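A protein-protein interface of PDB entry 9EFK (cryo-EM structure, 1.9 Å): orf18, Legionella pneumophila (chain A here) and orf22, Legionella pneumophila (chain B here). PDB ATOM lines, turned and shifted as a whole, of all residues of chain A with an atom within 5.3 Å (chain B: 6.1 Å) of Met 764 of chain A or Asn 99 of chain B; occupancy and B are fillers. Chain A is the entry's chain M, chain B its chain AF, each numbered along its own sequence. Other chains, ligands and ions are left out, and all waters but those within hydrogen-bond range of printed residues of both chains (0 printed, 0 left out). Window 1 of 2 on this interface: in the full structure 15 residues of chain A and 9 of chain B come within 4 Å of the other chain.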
ATOM      1  N   ASP A 682      10.748  -8.978 -24.065  1.00  0.00           N
ATOM      2  CA  ASP A 682      10.691  -9.921 -22.957  1.00  0.00           C
ATOM      3  C   ASP A 682       9.441  -9.756 -22.106  1.00  0.00           C
ATOM      4  O   ASP A 682       9.164 -10.623 -21.273  1.00  0.00           O
ATOM      5  CB  ASP A 682      11.925  -9.773 -22.072  1.00  0.00           C
ATOM      6  CG  ASP A 682      13.206 -10.030 -22.820  1.00  0.00           C
ATOM      7  OD1 ASP A 682      13.187 -10.847 -23.763  1.00  0.00           O
ATOM      8  OD2 ASP A 682      14.232  -9.415 -22.468  1.00  0.00           O
ATOM      9  N   ALA A 684       8.471  -6.686 -20.292  1.00  0.00           N
ATOM     10  CA  ALA A 684       8.645  -5.785 -19.163  1.00  0.00           C
ATOM     11  C   ALA A 684       8.284  -4.375 -19.597  1.00  0.00           C
ATOM     12  O   ALA A 684       8.793  -3.884 -20.606  1.00  0.00           O
ATOM     13  CB  ALA A 684      10.077  -5.828 -18.633  1.00  0.00           C
ATOM     14  N   PRO A 762       4.219  -7.198  -5.008  1.00  0.00           N
ATOM     15  CA  PRO A 762       5.534  -7.325  -5.644  1.00  0.00           C
ATOM     16  C   PRO A 762       5.568  -8.434  -6.683  1.00  0.00           C
ATOM     17  O   PRO A 762       4.847  -9.429  -6.592  1.00  0.00           O
ATOM     18  CB  PRO A 762       6.467  -7.643  -4.471  1.00  0.00           C
ATOM     19  CG  PRO A 762       5.697  -7.284  -3.243  1.00  0.00           C
ATOM     20  CD  PRO A 762       4.270  -7.519  -3.575  1.00  0.00           C
ATOM     21  N   ASN A 763       6.418  -8.243  -7.688  1.00  0.00           N
ATOM     22  CA  ASN A 763       6.698  -9.264  -8.693  1.00  0.00           C
ATOM     23  C   ASN A 763       8.195  -9.324  -8.978  1.00  0.00           C
ATOM     24  O   ASN A 763       8.638  -9.267 -10.124  1.00  0.00           O
ATOM     25  CB  ASN A 763       5.904  -9.032  -9.978  1.00  0.00           C
ATOM     26  CG  ASN A 763       5.839  -7.575 -10.381  1.00  0.00           C
ATOM     27  OD1 ASN A 763       4.777  -6.966 -10.353  1.00  0.00           O
ATOM     28  ND2 ASN A 763       6.969  -7.015 -10.774  1.00  0.00           N
ATOM     29  N   MET A 764       9.000  -9.419  -7.923  1.00  0.00           N
ATOM     30  CA  MET A 764      10.438  -9.596  -8.074  1.00  0.00           C
ATOM     31  C   MET A 764      10.972 -10.294  -6.835  1.00  0.00           C
ATOM     32  O   MET A 764      10.756  -9.819  -5.719  1.00  0.00           O
ATOM     33  CB  MET A 764      11.146  -8.256  -8.284  1.00  0.00           C
ATOM     34  CG  MET A 764      12.660  -8.350  -8.316  1.00  0.00           C
ATOM     35  SD  MET A 764      13.443  -6.796  -8.780  1.00  0.00           S
ATOM     36  CE  MET A 764      12.957  -6.679 -10.495  1.00  0.00           C
ATOM     37  N   HIS A 765      11.664 -11.409  -7.031  1.00  0.00           N
ATOM     38  CA  HIS A 765      12.160 -12.223  -5.926  1.00  0.00           C
ATOM     39  C   HIS A 765      13.596 -11.822  -5.624  1.00  0.00           C
ATOM     40  O   HIS A 765      14.528 -12.248  -6.305  1.00  0.00           O
ATOM     41  CB  HIS A 765      12.059 -13.706  -6.253  1.00  0.00           C
ATOM     42  CG  HIS A 765      10.663 -14.168  -6.518  1.00  0.00           C
ATOM     43  ND1 HIS A 765       9.686 -14.173  -5.547  1.00  0.00           N
ATOM     44  CD2 HIS A 765      10.078 -14.638  -7.644  1.00  0.00           C
ATOM     45  CE1 HIS A 765       8.559 -14.627  -6.064  1.00  0.00           C
ATOM     46  NE2 HIS A 765       8.770 -14.916  -7.335  1.00  0.00           N
ATOM     47  N   LEU A 766      13.771 -11.002  -4.595  1.00  0.00           N
ATOM     48  CA  LEU A 766      15.108 -10.664  -4.139  1.00  0.00           C
ATOM     49  C   LEU A 766      15.810 -11.921  -3.649  1.00  0.00           C
ATOM     50  O   LEU A 766      15.248 -12.694  -2.872  1.00  0.00           O
ATOM     51  CB  LEU A 766      15.030  -9.621  -3.028  1.00  0.00           C
ATOM     52  CG  LEU A 766      16.336  -9.071  -2.464  1.00  0.00           C
ATOM     53  CD1 LEU A 766      17.125  -8.361  -3.543  1.00  0.00           C
ATOM     54  CD2 LEU A 766      16.036  -8.136  -1.315  1.00  0.00           C
ATOM     55  N   TYR A 769      16.891 -13.306  -8.427  1.00  0.00           N
ATOM     56  CA  TYR A 769      16.672 -12.489  -9.608  1.00  0.00           C
ATOM     57  C   TYR A 769      18.016 -12.061 -10.165  1.00  0.00           C
ATOM     58  O   TYR A 769      18.870 -11.579  -9.418  1.00  0.00           O
ATOM     59  CB  TYR A 769      15.818 -11.259  -9.287  1.00  0.00           C
ATOM     60  CG  TYR A 769      15.756 -10.273 -10.421  1.00  0.00           C
ATOM     61  CD1 TYR A 769      14.919 -10.487 -11.502  1.00  0.00           C
ATOM     62  CD2 TYR A 769      16.543  -9.135 -10.417  1.00  0.00           C
ATOM     63  CE1 TYR A 769      14.868  -9.600 -12.542  1.00  0.00           C
ATOM     64  CE2 TYR A 769      16.496  -8.240 -11.452  1.00  0.00           C
ATOM     65  CZ  TYR A 769      15.654  -8.475 -12.511  1.00  0.00           C
ATOM     66  OH  TYR A 769      15.603  -7.586 -13.547  1.00  0.00           O
ATOM     67  N   GLY A 772      18.857  -7.506 -15.272  1.00  0.00           N
ATOM     68  CA  GLY A 772      18.689  -7.447 -16.701  1.00  0.00           C
ATOM     69  C   GLY A 772      17.589  -8.334 -17.241  1.00  0.00           C
ATOM     70  O   GLY A 772      17.135  -8.113 -18.367  1.00  0.00           O
ATOM     71  N   GLN A 773      17.147  -9.318 -16.472  1.00  0.00           N
ATOM     72  CA  GLN A 773      16.111 -10.235 -16.913  1.00  0.00           C
ATOM     73  C   GLN A 773      14.731  -9.700 -16.548  1.00  0.00           C
ATOM     74  O   GLN A 773      14.568  -8.915 -15.615  1.00  0.00           O
ATOM     75  CB  GLN A 773      16.320 -11.614 -16.292  1.00  0.00           C
ATOM     76  CG  GLN A 773      17.666 -12.230 -16.609  1.00  0.00           C
ATOM     77  CD  GLN A 773      17.891 -12.412 -18.093  1.00  0.00           C
ATOM     78  OE1 GLN A 773      17.100 -13.058 -18.774  1.00  0.00           O
ATOM     79  NE2 GLN A 773      18.969 -11.839 -18.602  1.00  0.00           N
ATOM     80  N   SER A 774      13.732 -10.132 -17.303  1.00  0.00           N
ATOM     81  CA  SER A 774      12.345  -9.779 -17.035  1.00  0.00           C
ATOM     82  C   SER A 774      11.683 -10.932 -16.295  1.00  0.00           C
ATOM     83  O   SER A 774      11.616 -12.046 -16.820  1.00  0.00           O
ATOM     84  CB  SER A 774      11.596  -9.482 -18.332  1.00  0.00           C
ATOM     85  OG  SER A 774      12.241  -8.461 -19.062  1.00  0.00           O
ATOM     86  N   VAL A 775      11.210 -10.674 -15.085  1.00  0.00           N
ATOM     87  CA  VAL A 775      10.527 -11.746 -14.355  1.00  0.00           C
ATOM     88  C   VAL A 775       9.209 -12.058 -15.055  1.00  0.00           C
ATOM     89  O   VAL A 775       8.465 -11.130 -15.415  1.00  0.00           O
ATOM     90  CB  VAL A 775      10.318 -11.360 -12.882  1.00  0.00           C
ATOM     91  CG1 VAL A 775      10.696  -9.927 -12.637  1.00  0.00           C
ATOM     92  CG2 VAL A 775       8.897 -11.638 -12.420  1.00  0.00           C
ATOM     93  N   ILE B  97       8.637  -2.848 -10.184  1.00  0.00           N
ATOM     94  CA  ILE B  97       9.463  -3.126 -11.349  1.00  0.00           C
ATOM     95  C   ILE B  97       9.535  -4.626 -11.581  1.00  0.00           C
ATOM     96  O   ILE B  97       9.571  -5.421 -10.634  1.00  0.00           O
ATOM     97  CB  ILE B  97      10.868  -2.532 -11.162  1.00  0.00           C
ATOM     98  CG1 ILE B  97      11.435  -2.948  -9.806  1.00  0.00           C
ATOM     99  CG2 ILE B  97      10.829  -1.033 -11.288  1.00  0.00           C
ATOM    100  CD1 ILE B  97      12.853  -2.508  -9.583  1.00  0.00           C
ATOM    101  N   SER B  98       9.547  -5.024 -12.851  1.00  0.00           N
ATOM    102  CA  SER B  98       9.806  -6.406 -13.226  1.00  0.00           C
ATOM    103  C   SER B  98      11.080  -6.540 -14.044  1.00  0.00           C
ATOM    104  O   SER B  98      11.338  -7.608 -14.603  1.00  0.00           O
ATOM    105  CB  SER B  98       8.626  -6.990 -14.003  1.00  0.00           C
ATOM    106  OG  SER B  98       8.610  -6.502 -15.326  1.00  0.00           O
ATOM    107  N   ASN B  99      11.876  -5.481 -14.141  1.00  0.00           N
ATOM    108  CA  ASN B  99      13.151  -5.535 -14.846  1.00  0.00           C
ATOM    109  C   ASN B  99      14.033  -4.442 -14.265  1.00  0.00           C
ATOM    110  O   ASN B  99      13.757  -3.256 -14.454  1.00  0.00           O
ATOM    111  CB  ASN B  99      12.965  -5.361 -16.349  1.00  0.00           C
ATOM    112  CG  ASN B  99      14.227  -5.656 -17.130  1.00  0.00           C
ATOM    113  OD1 ASN B  99      15.289  -5.117 -16.843  1.00  0.00           O
ATOM    114  ND2 ASN B  99      14.118  -6.530 -18.115  1.00  0.00           N
ATOM    115  N   LEU B 100      15.077  -4.844 -13.556  1.00  0.00           N
ATOM    116  CA  LEU B 100      16.023  -3.930 -12.928  1.00  0.00           C
ATOM    117  C   LEU B 100      17.393  -4.190 -13.537  1.00  0.00           C
ATOM    118  O   LEU B 100      18.025  -5.207 -13.240  1.00  0.00           O
ATOM    119  CB  LEU B 100      16.037  -4.124 -11.415  1.00  0.00           C
ATOM    120  CG  LEU B 100      17.042  -3.303 -10.616  1.00  0.00           C
ATOM    121  CD1 LEU B 100      16.817  -1.828 -10.848  1.00  0.00           C
ATOM    122  CD2 LEU B 100      16.927  -3.636  -9.145  1.00  0.00           C
ATOM    123  N   THR B 101      17.842  -3.277 -14.386  1.00  0.00           N
ATOM    124  CA  THR B 101      19.082  -3.458 -15.122  1.00  0.00           C
ATOM    125  C   THR B 101      20.285  -3.183 -14.226  1.00  0.00           C
ATOM    126  O   THR B 101      20.204  -2.429 -13.256  1.00  0.00           O
ATOM    127  CB  THR B 101      19.103  -2.537 -16.342  1.00  0.00           C
ATOM    128  OG1 THR B 101      17.892  -2.714 -17.084  1.00  0.00           O
ATOM    129  CG2 THR B 101      20.263  -2.859 -17.249  1.00  0.00           C
ATOM    130  N   ASP B 104      21.104   0.502 -14.223  1.00  0.00           N
ATOM    131  CA  ASP B 104      20.262   1.309 -13.348  1.00  0.00           C
ATOM    132  C   ASP B 104      20.697   1.183 -11.896  1.00  0.00           C
ATOM    133  O   ASP B 104      20.803   2.184 -11.182  1.00  0.00           O
ATOM    134  CB  ASP B 104      18.799   0.906 -13.501  1.00  0.00           C
ATOM    135  CG  ASP B 104      18.169   1.480 -14.743  1.00  0.00           C
ATOM    136  OD1 ASP B 104      18.840   2.270 -15.437  1.00  0.00           O
ATOM    137  OD2 ASP B 104      16.999   1.146 -15.026  1.00  0.00           O
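The side-chain amide nitrogen (ND2) of Asn 763 of chain A is in hydrogen-bond range of the backbone carbonyl oxygen (O) of Ile 97 of chain B, at 3.1 Å.
The backbone NH of Leu 100 of chain B is in hydrogen-bond range of the side-chain hydroxyl of Tyr 769 of chain A, 2.8 Å away.
The side-chain amide nitrogen (ND2) of Asn 99 of chain B sits at hydrogen-bond distance from the backbone carbonyl oxygen (O) of Gly 772 of chain A, at 3.4 Å.
The backbone NH of Gly 772 of chain A lies within hydrogen-bond range of the backbone carbonyl oxygen of Leu 100 of chain B.
The side-chain amide nitrogen of Asn 99 of chain B is in hydrogen-bond range of the backbone carbonyl oxygen of Gln 773 of chain A, at 3.5 Å.
The side-chain hydroxyl (OG) of Ser 774 of chain A sits at hydrogen-bond distance from the side-chain amide nitrogen (ND2) of Asn 99 of chain B, at 2.9 Å.
The backbone NH (N) of Val 775 of chain A sits at hydrogen-bond distance from the backbone carbonyl oxygen (O) of Ser 98 of chain B (3.1 Å).
O of Gln 773 of chain A lies within hydrogen-bond range of OH of Tyr 769 of chain A (2.7 Å).
Among the printed residues, pairs that only touch across the chains: Ser 774 of chain A with Ser 98 of chain B (3.4 Å), Tyr 769 of chain A with Asn 99 of chain B (3.5 Å), Met 764 of chain A with Ile 97 of chain B (3.6 Å), Gln 773 of chain A with Ser 98 of chain B (3.6 Å), Asn 763 of chain A with Ser 98 of chain B (3.6 Å), Ala 684 of chain A with Ser 98 of chain B (3.7 Å), Ala 684 of chain A with Asn 99 of chain B (3.7 Å) and Met 764 of chain A with Asn 99 of chain B (3.99 Å).
Printed residues of chain B within 4 Å of Ala 684 of chain A: Ser 98 (3.7 Å) and Asn 99 (3.7 Å).
Pro 762 of chain A touches none of the printed residues of chain B.
Of the printed residues of chain B, Asn 763 of chain A touches Ile 97 and Ser 98.
Of the printed residues of chain B, Tyr 769 of chain A touches Asn 99 and Leu 100.
Of the printed residues of chain A, Asn 99 of chain B touches Ala 684 (3.7 Å), Met 764 (3.99 Å), Tyr 769 (3.5 Å), Gly 772 (3.4 Å), Gln 773 (3.5 Å) and Ser 774 (2.9 Å).
Of the printed residues of chain A, Leu 100 of chain B touches Tyr 769 (2.8 Å) and Gly 772 (3.2 Å).
The nearest printed residue of chain B that does not touch Met 764 of chain A is Ser 98 of chain B (4.02 Å).
The nearest printed residue of chain B that does not touch Gln 773 of chain A is Leu 100 of chain B (4.6 Å).
Of the 6 printed residues of chain B, 4 touch a printed residue of chain A.
Printed residues of chain B that touch a printed residue of chain A: Ile 97, Ser 98, Asn 99 and Leu 100.
Hydrophobic or aromatic side chains of chain A within 4 Å of the printed part of chain B: Ala 684, Met 764, Tyr 769 and Val 775.
Along chain A the printed residues that touch a printed residue of chain B span positions 684 to 775.
Among the printed residues, no Asp or Glu carboxylate lies within 4 Å of a Lys or Arg side-chain nitrogen of the other chain.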
